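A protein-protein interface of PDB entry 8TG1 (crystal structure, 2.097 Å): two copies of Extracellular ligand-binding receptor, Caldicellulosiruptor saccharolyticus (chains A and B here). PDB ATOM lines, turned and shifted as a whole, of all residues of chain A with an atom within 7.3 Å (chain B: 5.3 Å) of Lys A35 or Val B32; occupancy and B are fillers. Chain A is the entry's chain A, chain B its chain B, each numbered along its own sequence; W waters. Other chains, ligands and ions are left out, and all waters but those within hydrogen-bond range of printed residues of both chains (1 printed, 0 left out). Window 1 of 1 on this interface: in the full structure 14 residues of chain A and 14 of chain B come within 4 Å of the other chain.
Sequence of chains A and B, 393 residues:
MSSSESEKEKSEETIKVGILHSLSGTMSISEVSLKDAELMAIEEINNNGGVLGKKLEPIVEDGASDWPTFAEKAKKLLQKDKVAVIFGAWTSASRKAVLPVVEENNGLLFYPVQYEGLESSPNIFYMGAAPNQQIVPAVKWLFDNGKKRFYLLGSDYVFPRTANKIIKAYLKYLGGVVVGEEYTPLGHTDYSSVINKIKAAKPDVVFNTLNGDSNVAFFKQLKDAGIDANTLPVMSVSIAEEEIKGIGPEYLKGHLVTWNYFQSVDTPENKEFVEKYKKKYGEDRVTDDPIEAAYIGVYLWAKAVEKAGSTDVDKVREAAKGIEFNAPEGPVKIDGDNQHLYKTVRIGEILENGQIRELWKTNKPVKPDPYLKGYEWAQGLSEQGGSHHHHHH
Among the printed residues, pairs that only touch across the chains: Leu A23 with Leu B23 (3.6 Å), Val A32 with Lys B35 (3.95 Å), Lys A35 with Val B32 (3.8 Å) and Leu A39 with Ser B24 (3.7 Å).
Leu B23 touches its own counterpart, Leu A23. Leu A23 touches Lys B35, and with the chains exchanged Lys A35 touches Leu B23. Val A32 touches Lys B35, and with the chains exchanged Lys A35 touches Val B32. 8 positions are printed for both chains. Of the 6 pairs that touch across the chains among the printed residues, 5 have their exchanged pair printed and touching as well.
Printed residues of chain B that touch a printed residue of chain A: Leu B23, Ser B24, Val B32 and Lys B35. Hydrophobic or aromatic side chains of chain B within 4 Å of the printed part of chain A: Leu B23 and Val B32. Along chain B the printed residues that touch a printed residue of chain A span positions 23 to 35. Printed residues of chain A that touch a printed residue of chain B: Leu A23, Val A32, Lys A35 and Leu A39. Hydrophobic or aromatic side chains of chain A that line the printed part of chain B: Leu A23, Val A32 and Leu A39. Among the printed residues, 6 pairs touch across the chains. Among the printed residues, no Asp or Glu carboxylate lies within 4 Å of a Lys or Arg side-chain nitrogen of the other chain.
The backbone carbonyl oxygen of Leu A23 is in hydrogen-bond range of the side-chain amino group of Lys B35, 2.9 Å away. The side-chain amino group of Lys A35 sits at hydrogen-bond distance from the backbone carbonyl oxygen of Leu B23 (2.9 Å).
Water W1 bridges OD1 of Asp B36 and O of Leu A23.
The side-chain amino group (NZ) of Lys A35 is in salt-bridge range of the side-chain carboxylate (OD1) of Asp A36, 3.4 Å away. The side-chain carboxylate (OD1) of Asp B36 is in salt-bridge range of the side-chain amino group (NZ) of Lys B35 (3.3 Å).
Ile A19 touches none of the printed residues of chain B. Lys A35 touches just these residues of chain B: Leu B23 and Val B32. Of the printed residues of chain B, Leu A39 touches Ser B24 (3.7 Å). Of the printed residues of chain A, Ser B24 touches Leu A39. Ser B28 touches none of the printed residues of chain A. Val B32 touches just one residue of chain A: Lys A35. The nearest residue of chain A that does not touch Val B32 is Val A32 (4.8 Å). The nearest printed residue of chain B that does not touch Val A32 is Val B32 (4.8 Å).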
ATOM      1  N   ILE A  19      -2.707  -0.069 -14.190  1.00  0.00           N
ATOM      2  CA  ILE A  19      -3.648  -0.920 -14.905  1.00  0.00           C
ATOM      3  C   ILE A  19      -3.256  -0.881 -16.374  1.00  0.00           C
ATOM      4  O   ILE A  19      -3.284   0.186 -17.001  1.00  0.00           O
ATOM      5  CB  ILE A  19      -5.104  -0.468 -14.705  1.00  0.00           C
ATOM      6  CG1 ILE A  19      -5.537  -0.698 -13.254  1.00  0.00           C
ATOM      7  CG2 ILE A  19      -6.029  -1.204 -15.663  1.00  0.00           C
ATOM      8  CD1 ILE A  19      -6.966  -0.281 -12.968  1.00  0.00           C
ATOM      9  N   LEU A  20      -2.886  -2.037 -16.921  1.00  0.00           N
ATOM     10  CA  LEU A  20      -2.307  -2.128 -18.259  1.00  0.00           C
ATOM     11  C   LEU A  20      -3.059  -3.197 -19.047  1.00  0.00           C
ATOM     12  O   LEU A  20      -2.733  -4.384 -18.962  1.00  0.00           O
ATOM     13  CB  LEU A  20      -0.815  -2.439 -18.177  1.00  0.00           C
ATOM     14  CG  LEU A  20      -0.042  -2.642 -19.478  1.00  0.00           C
ATOM     15  CD1 LEU A  20      -0.370  -1.538 -20.459  1.00  0.00           C
ATOM     16  CD2 LEU A  20       1.449  -2.673 -19.191  1.00  0.00           C
ATOM     17  N   HIS A  21      -4.051  -2.779 -19.829  1.00  0.00           N
ATOM     18  CA  HIS A  21      -4.882  -3.708 -20.581  1.00  0.00           C
ATOM     19  C   HIS A  21      -5.122  -3.174 -21.984  1.00  0.00           C
ATOM     20  O   HIS A  21      -4.969  -1.981 -22.255  1.00  0.00           O
ATOM     21  CB  HIS A  21      -6.227  -3.951 -19.886  1.00  0.00           C
ATOM     22  CG  HIS A  21      -6.154  -4.897 -18.728  1.00  0.00           C
ATOM     23  ND1 HIS A  21      -5.824  -6.226 -18.872  1.00  0.00           N
ATOM     24  CD2 HIS A  21      -6.369  -4.704 -17.405  1.00  0.00           C
ATOM     25  CE1 HIS A  21      -5.844  -6.813 -17.690  1.00  0.00           C
ATOM     26  NE2 HIS A  21      -6.168  -5.911 -16.781  1.00  0.00           N
ATOM     27  N   LEU A  23      -7.326  -1.750 -24.195  1.00  0.00           N
ATOM     28  CA  LEU A  23      -8.589  -1.039 -24.308  1.00  0.00           C
ATOM     29  C   LEU A  23      -8.958  -0.753 -25.755  1.00  0.00           C
ATOM     30  O   LEU A  23     -10.071  -0.288 -26.022  1.00  0.00           O
ATOM     31  CB  LEU A  23      -8.529   0.263 -23.508  1.00  0.00           C
ATOM     32  CG  LEU A  23      -7.845   0.108 -22.147  1.00  0.00           C
ATOM     33  CD1 LEU A  23      -7.709   1.444 -21.446  1.00  0.00           C
ATOM     34  CD2 LEU A  23      -8.603  -0.881 -21.274  1.00  0.00           C
ATOM     35  N   SER A  30     -12.012  -8.645 -24.683  1.00  0.00           N
ATOM     36  CA  SER A  30     -11.714  -9.442 -23.502  1.00  0.00           C
ATOM     37  C   SER A  30     -11.207  -8.617 -22.327  1.00  0.00           C
ATOM     38  O   SER A  30     -11.560  -8.906 -21.181  1.00  0.00           O
ATOM     39  CB  SER A  30     -10.667 -10.511 -23.841  1.00  0.00           C
ATOM     40  OG  SER A  30     -11.237 -11.577 -24.581  1.00  0.00           O
ATOM     41  N   GLU A  31     -10.392  -7.591 -22.584  1.00  0.00           N
ATOM     42  CA  GLU A  31      -9.592  -6.968 -21.538  1.00  0.00           C
ATOM     43  C   GLU A  31     -10.233  -5.751 -20.885  1.00  0.00           C
ATOM     44  O   GLU A  31      -9.861  -5.417 -19.754  1.00  0.00           O
ATOM     45  CB  GLU A  31      -8.224  -6.557 -22.093  1.00  0.00           C
ATOM     46  CG  GLU A  31      -7.373  -7.727 -22.533  1.00  0.00           C
ATOM     47  CD  GLU A  31      -5.913  -7.357 -22.677  1.00  0.00           C
ATOM     48  OE1 GLU A  31      -5.375  -6.699 -21.760  1.00  0.00           O
ATOM     49  OE2 GLU A  31      -5.306  -7.724 -23.705  1.00  0.00           O
ATOM     50  N   VAL A  32     -11.162  -5.073 -21.561  1.00  0.00           N
ATOM     51  CA  VAL A  32     -11.763  -3.877 -20.978  1.00  0.00           C
ATOM     52  C   VAL A  32     -12.483  -4.222 -19.681  1.00  0.00           C
ATOM     53  O   VAL A  32     -12.395  -3.485 -18.690  1.00  0.00           O
ATOM     54  CB  VAL A  32     -12.708  -3.200 -21.992  1.00  0.00           C
ATOM     55  CG1 VAL A  32     -13.482  -2.062 -21.333  1.00  0.00           C
ATOM     56  CG2 VAL A  32     -11.923  -2.689 -23.190  1.00  0.00           C
ATOM     57  N   SER A  33     -13.187  -5.355 -19.655  1.00  0.00           N
ATOM     58  CA  SER A  33     -13.895  -5.752 -18.444  1.00  0.00           C
ATOM     59  C   SER A  33     -12.946  -6.082 -17.300  1.00  0.00           C
ATOM     60  O   SER A  33     -13.353  -6.011 -16.136  1.00  0.00           O
ATOM     61  CB  SER A  33     -14.801  -6.947 -18.732  1.00  0.00           C
ATOM     62  OG  SER A  33     -14.069  -7.990 -19.345  1.00  0.00           O
ATOM     63  N   LEU A  34     -11.694  -6.445 -17.600  1.00  0.00           N
ATOM     64  CA  LEU A  34     -10.723  -6.661 -16.530  1.00  0.00           C
ATOM     65  C   LEU A  34     -10.330  -5.344 -15.875  1.00  0.00           C
ATOM     66  O   LEU A  34     -10.099  -5.294 -14.661  1.00  0.00           O
ATOM     67  CB  LEU A  34      -9.485  -7.384 -17.063  1.00  0.00           C
ATOM     68  CG  LEU A  34      -9.682  -8.742 -17.740  1.00  0.00           C
ATOM     69  CD1 LEU A  34      -8.363  -9.506 -17.787  1.00  0.00           C
ATOM     70  CD2 LEU A  34     -10.755  -9.557 -17.039  1.00  0.00           C
ATOM     71  N   LYS A  35     -10.242  -4.270 -16.663  1.00  0.00           N
ATOM     72  CA  LYS A  35     -10.042  -2.944 -16.087  1.00  0.00           C
ATOM     73  C   LYS A  35     -11.212  -2.562 -15.190  1.00  0.00           C
ATOM     74  O   LYS A  35     -11.020  -1.965 -14.123  1.00  0.00           O
ATOM     75  CB  LYS A  35      -9.850  -1.911 -17.199  1.00  0.00           C
ATOM     76  CG  LYS A  35      -9.809  -0.468 -16.716  1.00  0.00           C
ATOM     77  CD  LYS A  35     -10.502   0.465 -17.697  1.00  0.00           C
ATOM     78  CE  LYS A  35     -11.975   0.121 -17.832  1.00  0.00           C
ATOM     79  NZ  LYS A  35     -12.750   1.185 -18.531  1.00  0.00           N
ATOM     80  N   ASP A  36     -12.437  -2.904 -15.605  1.00  0.00           N
ATOM     81  CA  ASP A  36     -13.606  -2.649 -14.770  1.00  0.00           C
ATOM     82  C   ASP A  36     -13.523  -3.416 -13.457  1.00  0.00           C
ATOM     83  O   ASP A  36     -13.880  -2.889 -12.396  1.00  0.00           O
ATOM     84  CB  ASP A  36     -14.885  -3.028 -15.521  1.00  0.00           C
ATOM     85  CG  ASP A  36     -15.147  -2.140 -16.722  1.00  0.00           C
ATOM     86  OD1 ASP A  36     -14.700  -0.974 -16.706  1.00  0.00           O
ATOM     87  OD2 ASP A  36     -15.810  -2.607 -17.676  1.00  0.00           O
ATOM     88  N   ALA A  37     -13.060  -4.666 -13.511  1.00  0.00           N
ATOM     89  CA  ALA A  37     -12.969  -5.480 -12.305  1.00  0.00           C
ATOM     90  C   ALA A  37     -11.910  -4.932 -11.356  1.00  0.00           C
ATOM     91  O   ALA A  37     -12.143  -4.818 -10.148  1.00  0.00           O
ATOM     92  CB  ALA A  37     -12.670  -6.933 -12.671  1.00  0.00           C
ATOM     93  N   GLU A  38     -10.739  -4.584 -11.893  1.00  0.00           N
ATOM     94  CA  GLU A  38      -9.672  -4.042 -11.055  1.00  0.00           C
ATOM     95  C   GLU A  38     -10.074  -2.705 -10.446  1.00  0.00           C
ATOM     96  O   GLU A  38      -9.770  -2.429  -9.280  1.00  0.00           O
ATOM     97  CB  GLU A  38      -8.387  -3.901 -11.869  1.00  0.00           C
ATOM     98  CG  GLU A  38      -7.796  -5.225 -12.322  1.00  0.00           C
ATOM     99  CD  GLU A  38      -7.142  -5.134 -13.685  1.00  0.00           C
ATOM    100  OE1 GLU A  38      -7.091  -4.018 -14.246  1.00  0.00           O
ATOM    101  OE2 GLU A  38      -6.686  -6.178 -14.196  1.00  0.00           O
ATOM    102  N   LEU A  39     -10.769  -1.864 -11.216  1.00  0.00           N
ATOM    103  CA  LEU A  39     -11.208  -0.576 -10.688  1.00  0.00           C
ATOM    104  C   LEU A  39     -12.269  -0.740  -9.606  1.00  0.00           C
ATOM    105  O   LEU A  39     -12.314   0.060  -8.664  1.00  0.00           O
ATOM    106  CB  LEU A  39     -11.729   0.308 -11.822  1.00  0.00           C
ATOM    107  CG  LEU A  39     -10.657   0.962 -12.696  1.00  0.00           C
ATOM    108  CD1 LEU A  39     -11.308   1.708 -13.854  1.00  0.00           C
ATOM    109  CD2 LEU A  39      -9.774   1.893 -11.881  1.00  0.00           C
ATOM    110  N   MET A  40     -13.122  -1.763  -9.714  1.00  0.00           N
ATOM    111  CA  MET A  40     -14.127  -1.983  -8.679  1.00  0.00           C
ATOM    112  C   MET A  40     -13.477  -2.435  -7.379  1.00  0.00           C
ATOM    113  O   MET A  40     -13.838  -1.952  -6.299  1.00  0.00           O
ATOM    114  CB  MET A  40     -15.167  -3.001  -9.158  1.00  0.00           C
ATOM    115  CG  MET A  40     -16.309  -3.250  -8.175  1.00  0.00           C
ATOM    116  SD  MET A  40     -17.389  -4.631  -8.621  1.00  0.00           S
ATOM    117  CE  MET A  40     -16.583  -6.021  -7.843  1.00  0.00           C
ATOM    118  N   ALA A  41     -12.495  -3.334  -7.466  1.00  0.00           N
ATOM    119  CA  ALA A  41     -11.791  -3.784  -6.270  1.00  0.00           C
ATOM    120  C   ALA A  41     -11.037  -2.638  -5.610  1.00  0.00           C
ATOM    121  O   ALA A  41     -10.996  -2.541  -4.378  1.00  0.00           O
ATOM    122  CB  ALA A  41     -10.836  -4.924  -6.621  1.00  0.00           C
ATOM    123  N   ILE A  42     -10.434  -1.759  -6.415  1.00  0.00           N
ATOM    124  CA  ILE A  42      -9.716  -0.615  -5.863  1.00  0.00           C
ATOM    125  C   ILE A  42     -10.674   0.315  -5.130  1.00  0.00           C
ATOM    126  O   ILE A  42     -10.369   0.809  -4.036  1.00  0.00           O
ATOM    127  CB  ILE A  42      -8.949   0.123  -6.976  1.00  0.00           C
ATOM    128  CG1 ILE A  42      -7.829  -0.759  -7.530  1.00  0.00           C
ATOM    129  CG2 ILE A  42      -8.386   1.430  -6.450  1.00  0.00           C
ATOM    130  CD1 ILE A  42      -7.255  -0.264  -8.845  1.00  0.00           C
ATOM    131  N   VAL A  60      -4.302   4.155 -15.517  1.00  0.00           N
ATOM    132  CA  VAL A  60      -4.822   3.265 -16.546  1.00  0.00           C
ATOM    133  C   VAL A  60      -4.107   3.552 -17.858  1.00  0.00           C
ATOM    134  O   VAL A  60      -4.062   4.702 -18.312  1.00  0.00           O
ATOM    135  CB  VAL A  60      -6.344   3.430 -16.701  1.00  0.00           C
ATOM    136  CG1 VAL A  60      -6.859   2.570 -17.845  1.00  0.00           C
ATOM    137  CG2 VAL A  60      -7.047   3.091 -15.391  1.00  0.00           C
ATOM    138  N   GLU A  61      -3.552   2.507 -18.471  1.00  0.00           N
ATOM    139  CA  GLU A  61      -2.823   2.627 -19.724  1.00  0.00           C
ATOM    140  C   GLU A  61      -3.349   1.610 -20.725  1.00  0.00           C
ATOM    141  O   GLU A  61      -3.693   0.482 -20.359  1.00  0.00           O
ATOM    142  CB  GLU A  61      -1.318   2.423 -19.520  1.00  0.00           C
ATOM    143  CG  GLU A  61      -0.663   3.472 -18.642  1.00  0.00           C
ATOM    144  CD  GLU A  61      -0.635   4.847 -19.284  1.00  0.00           C
ATOM    145  OE1 GLU A  61      -0.650   4.928 -20.532  1.00  0.00           O
ATOM    146  OE2 GLU A  61      -0.605   5.848 -18.533  1.00  0.00           O
ATOM    147  N   PHE A  87      -1.460  -4.304 -12.547  1.00  0.00           N
ATOM    148  CA  PHE A  87      -2.449  -5.316 -12.885  1.00  0.00           C
ATOM    149  C   PHE A  87      -2.726  -5.211 -14.377  1.00  0.00           C
ATOM    150  O   PHE A  87      -3.087  -4.135 -14.862  1.00  0.00           O
ATOM    151  CB  PHE A  87      -3.742  -5.110 -12.091  1.00  0.00           C
ATOM    152  CG  PHE A  87      -3.534  -4.914 -10.610  1.00  0.00           C
ATOM    153  CD1 PHE A  87      -3.290  -5.996  -9.779  1.00  0.00           C
ATOM    154  CD2 PHE A  87      -3.592  -3.647 -10.049  1.00  0.00           C
ATOM    155  CE1 PHE A  87      -3.104  -5.821  -8.421  1.00  0.00           C
ATOM    156  CE2 PHE A  87      -3.408  -3.464  -8.691  1.00  0.00           C
ATOM    157  CZ  PHE A  87      -3.161  -4.551  -7.876  1.00  0.00           C
ATOM    158  N   TYR A 277     -20.931  -6.275  -8.872  1.00  0.00           N
ATOM    159  CA  TYR A 277     -20.477  -5.979 -10.228  1.00  0.00           C
ATOM    160  C   TYR A 277     -21.612  -5.410 -11.075  1.00  0.00           C
ATOM    161  O   TYR A 277     -21.417  -4.430 -11.805  1.00  0.00           O
ATOM    162  CB  TYR A 277     -19.899  -7.242 -10.869  1.00  0.00           C
ATOM    163  CG  TYR A 277     -19.068  -6.998 -12.112  1.00  0.00           C
ATOM    164  CD1 TYR A 277     -17.729  -6.638 -12.014  1.00  0.00           C
ATOM    165  CD2 TYR A 277     -19.618  -7.139 -13.382  1.00  0.00           C
ATOM    166  CE1 TYR A 277     -16.962  -6.417 -13.144  1.00  0.00           C
ATOM    167  CE2 TYR A 277     -18.858  -6.921 -14.518  1.00  0.00           C
ATOM    168  CZ  TYR A 277     -17.530  -6.562 -14.392  1.00  0.00           C
ATOM    169  OH  TYR A 277     -16.768  -6.341 -15.519  1.00  0.00           O
ATOM    170  N   TYR A 281     -21.889  -1.538 -12.686  1.00  0.00           N
ATOM    171  CA  TYR A 281     -21.759  -1.400 -14.129  1.00  0.00           C
ATOM    172  C   TYR A 281     -23.038  -1.677 -14.907  1.00  0.00           C
ATOM    173  O   TYR A 281     -23.070  -1.418 -16.114  1.00  0.00           O
ATOM    174  CB  TYR A 281     -20.647  -2.325 -14.644  1.00  0.00           C
ATOM    175  CG  TYR A 281     -19.284  -1.971 -14.098  1.00  0.00           C
ATOM    176  CD1 TYR A 281     -18.705  -0.738 -14.373  1.00  0.00           C
ATOM    177  CD2 TYR A 281     -18.585  -2.861 -13.291  1.00  0.00           C
ATOM    178  CE1 TYR A 281     -17.464  -0.405 -13.873  1.00  0.00           C
ATOM    179  CE2 TYR A 281     -17.342  -2.536 -12.784  1.00  0.00           C
ATOM    180  CZ  TYR A 281     -16.787  -1.306 -13.079  1.00  0.00           C
ATOM    181  OH  TYR A 281     -15.550  -0.972 -12.581  1.00  0.00           O
ATOM    182  N   ILE A 291     -12.439 -12.069 -15.174  1.00  0.00           N
ATOM    183  CA  ILE A 291     -12.936 -10.928 -14.408  1.00  0.00           C
ATOM    184  C   ILE A 291     -12.743 -11.165 -12.917  1.00  0.00           C
ATOM    185  O   ILE A 291     -12.294 -10.278 -12.181  1.00  0.00           O
ATOM    186  CB  ILE A 291     -14.411 -10.648 -14.751  1.00  0.00           C
ATOM    187  CG1 ILE A 291     -14.510 -10.008 -16.135  1.00  0.00           C
ATOM    188  CG2 ILE A 291     -15.055  -9.758 -13.697  1.00  0.00           C
ATOM    189  CD1 ILE A 291     -15.899 -10.080 -16.741  1.00  0.00           C
ATOM    190  N   ALA A 294      -8.955 -10.929 -12.085  1.00  0.00           N
ATOM    191  CA  ALA A 294      -8.522  -9.537 -11.998  1.00  0.00           C
ATOM    192  C   ALA A 294      -8.968  -8.908 -10.685  1.00  0.00           C
ATOM    193  O   ALA A 294      -8.203  -8.177 -10.044  1.00  0.00           O
ATOM    194  CB  ALA A 294      -9.067  -8.744 -13.186  1.00  0.00           C
ATOM    195  N   SER B  22     -12.604   9.722 -20.379  1.00  0.00           N
ATOM    196  CA  SER B  22     -12.581   9.157 -19.034  1.00  0.00           C
ATOM    197  C   SER B  22     -12.840   7.661 -19.128  1.00  0.00           C
ATOM    198  O   SER B  22     -13.983   7.221 -19.269  1.00  0.00           O
ATOM    199  CB  SER B  22     -13.616   9.831 -18.141  1.00  0.00           C
ATOM    200  OG  SER B  22     -13.373  11.221 -18.034  1.00  0.00           O
ATOM    201  N   LEU B  23     -11.772   6.871 -19.072  1.00  0.00           N
ATOM    202  CA  LEU B  23     -11.904   5.427 -18.979  1.00  0.00           C
ATOM    203  C   LEU B  23     -11.923   4.950 -17.534  1.00  0.00           C
ATOM    204  O   LEU B  23     -12.162   3.764 -17.289  1.00  0.00           O
ATOM    205  CB  LEU B  23     -10.775   4.739 -19.755  1.00  0.00           C
ATOM    206  CG  LEU B  23     -10.555   5.304 -21.163  1.00  0.00           C
ATOM    207  CD1 LEU B  23      -9.422   4.591 -21.873  1.00  0.00           C
ATOM    208  CD2 LEU B  23     -11.831   5.213 -21.986  1.00  0.00           C
ATOM    209  N   SER B  24     -11.680   5.849 -16.583  1.00  0.00           N
ATOM    210  CA  SER B  24     -11.805   5.566 -15.162  1.00  0.00           C
ATOM    211  C   SER B  24     -12.442   6.775 -14.493  1.00  0.00           C
ATOM    212  O   SER B  24     -12.463   7.874 -15.051  1.00  0.00           O
ATOM    213  CB  SER B  24     -10.446   5.249 -14.519  1.00  0.00           C
ATOM    214  OG  SER B  24      -9.551   6.340 -14.649  1.00  0.00           O
ATOM    215  N   MET B  27     -16.940   9.674 -14.519  1.00  0.00           N
ATOM    216  CA  MET B  27     -17.444   9.925 -15.862  1.00  0.00           C
ATOM    217  C   MET B  27     -17.367   8.705 -16.771  1.00  0.00           C
ATOM    218  O   MET B  27     -17.956   8.726 -17.859  1.00  0.00           O
ATOM    219  CB  MET B  27     -16.667  11.073 -16.517  1.00  0.00           C
ATOM    220  CG  MET B  27     -17.180  12.485 -16.229  1.00  0.00           C
ATOM    221  SD  MET B  27     -18.928  12.657 -15.817  1.00  0.00           S
ATOM    222  CE  MET B  27     -19.720  12.204 -17.357  1.00  0.00           C
ATOM    223  N   SER B  28     -16.648   7.655 -16.366  1.00  0.00           N
ATOM    224  CA  SER B  28     -16.390   6.526 -17.257  1.00  0.00           C
ATOM    225  C   SER B  28     -17.661   5.791 -17.659  1.00  0.00           C
ATOM    226  O   SER B  28     -17.669   5.114 -18.694  1.00  0.00           O
ATOM    227  CB  SER B  28     -15.408   5.555 -16.604  1.00  0.00           C
ATOM    228  OG  SER B  28     -15.990   4.925 -15.475  1.00  0.00           O
ATOM    229  N   ILE B  29     -18.731   5.897 -16.865  1.00  0.00           N
ATOM    230  CA  ILE B  29     -20.014   5.325 -17.264  1.00  0.00           C
ATOM    231  C   ILE B  29     -20.465   5.904 -18.598  1.00  0.00           C
ATOM    232  O   ILE B  29     -21.108   5.216 -19.402  1.00  0.00           O
ATOM    233  CB  ILE B  29     -21.066   5.554 -16.156  1.00  0.00           C
ATOM    234  CG1 ILE B  29     -22.423   4.973 -16.560  1.00  0.00           C
ATOM    235  CG2 ILE B  29     -21.205   7.041 -15.829  1.00  0.00           C
ATOM    236  CD1 ILE B  29     -23.506   5.159 -15.514  1.00  0.00           C
ATOM    237  N   SER B  30     -20.113   7.161 -18.870  1.00  0.00           N
ATOM    238  CA  SER B  30     -20.538   7.855 -20.080  1.00  0.00           C
ATOM    239  C   SER B  30     -19.516   7.766 -21.209  1.00  0.00           C
ATOM    240  O   SER B  30     -19.896   7.602 -22.373  1.00  0.00           O
ATOM    241  CB  SER B  30     -20.821   9.328 -19.765  1.00  0.00           C
ATOM    242  OG  SER B  30     -22.021   9.486 -19.028  1.00  0.00           O
ATOM    243  N   GLU B  31     -18.221   7.864 -20.893  1.00  0.00           N
ATOM    244  CA  GLU B  31     -17.210   8.138 -21.906  1.00  0.00           C
ATOM    245  C   GLU B  31     -16.588   6.897 -22.532  1.00  0.00           C
ATOM    246  O   GLU B  31     -16.011   7.002 -23.621  1.00  0.00           O
ATOM    247  CB  GLU B  31     -16.091   9.003 -21.318  1.00  0.00           C
ATOM    248  CG  GLU B  31     -16.538  10.403 -20.942  1.00  0.00           C
ATOM    249  CD  GLU B  31     -15.375  11.358 -20.755  1.00  0.00           C
ATOM    250  OE1 GLU B  31     -14.551  11.487 -21.684  1.00  0.00           O
ATOM    251  OE2 GLU B  31     -15.292  11.995 -19.685  1.00  0.00           O
ATOM    252  N   VAL B  32     -16.673   5.736 -21.882  1.00  0.00           N
ATOM    253  CA  VAL B  32     -16.032   4.544 -22.433  1.00  0.00           C
ATOM    254  C   VAL B  32     -16.640   4.185 -23.784  1.00  0.00           C
ATOM    255  O   VAL B  32     -15.922   3.852 -24.736  1.00  0.00           O
ATOM    256  CB  VAL B  32     -16.122   3.374 -21.436  1.00  0.00           C
ATOM    257  CG1 VAL B  32     -15.799   2.066 -22.134  1.00  0.00           C
ATOM    258  CG2 VAL B  32     -15.171   3.602 -20.273  1.00  0.00           C
ATOM    259  N   SER B  33     -17.969   4.264 -23.897  1.00  0.00           N
ATOM    260  CA  SER B  33     -18.620   3.931 -25.158  1.00  0.00           C
ATOM    261  C   SER B  33     -18.331   4.955 -26.248  1.00  0.00           C
ATOM    262  O   SER B  33     -18.540   4.655 -27.429  1.00  0.00           O
ATOM    263  CB  SER B  33     -20.130   3.791 -24.959  1.00  0.00           C
ATOM    264  OG  SER B  33     -20.687   4.975 -24.421  1.00  0.00           O
ATOM    265  N   LEU B  34     -17.859   6.152 -25.886  1.00  0.00           N
ATOM    266  CA  LEU B  34     -17.422   7.100 -26.906  1.00  0.00           C
ATOM    267  C   LEU B  34     -16.121   6.642 -27.549  1.00  0.00           C
ATOM    268  O   LEU B  34     -15.958   6.741 -28.771  1.00  0.00           O
ATOM    269  CB  LEU B  34     -17.266   8.498 -26.309  1.00  0.00           C
ATOM    270  CG  LEU B  34     -18.540   9.148 -25.766  1.00  0.00           C
ATOM    271  CD1 LEU B  34     -18.357  10.653 -25.611  1.00  0.00           C
ATOM    272  CD2 LEU B  34     -19.717   8.843 -26.669  1.00  0.00           C
ATOM    273  N   LYS B  35     -15.185   6.137 -26.741  1.00  0.00           N
ATOM    274  CA  LYS B  35     -13.972   5.541 -27.292  1.00  0.00           C
ATOM    275  C   LYS B  35     -14.308   4.380 -28.219  1.00  0.00           C
ATOM    276  O   LYS B  35     -13.672   4.205 -29.266  1.00  0.00           O
ATOM    277  CB  LYS B  35     -13.054   5.083 -26.159  1.00  0.00           C
ATOM    278  CG  LYS B  35     -11.902   4.201 -26.610  1.00  0.00           C
ATOM    279  CD  LYS B  35     -11.580   3.116 -25.590  1.00  0.00           C
ATOM    280  CE  LYS B  35     -12.781   2.236 -25.304  1.00  0.00           C
ATOM    281  NZ  LYS B  35     -12.395   0.892 -24.789  1.00  0.00           N
ATOM    282  N   ASP B  36     -15.316   3.583 -27.854  1.00  0.00           N
ATOM    283  CA  ASP B  36     -15.757   2.492 -28.716  1.00  0.00           C
ATOM    284  C   ASP B  36     -16.291   3.022 -30.039  1.00  0.00           C
ATOM    285  O   ASP B  36     -15.972   2.491 -31.111  1.00  0.00           O
ATOM    286  CB  ASP B  36     -16.826   1.658 -28.005  1.00  0.00           C
ATOM    287  CG  ASP B  36     -16.272   0.889 -26.819  1.00  0.00           C
ATOM    288  OD1 ASP B  36     -15.042   0.677 -26.776  1.00  0.00           O
ATOM    289  OD2 ASP B  36     -17.065   0.497 -25.934  1.00  0.00           O
HETATM  290  O   HOH W   1     -13.017  -0.944 -27.709  1.00  0.00           O
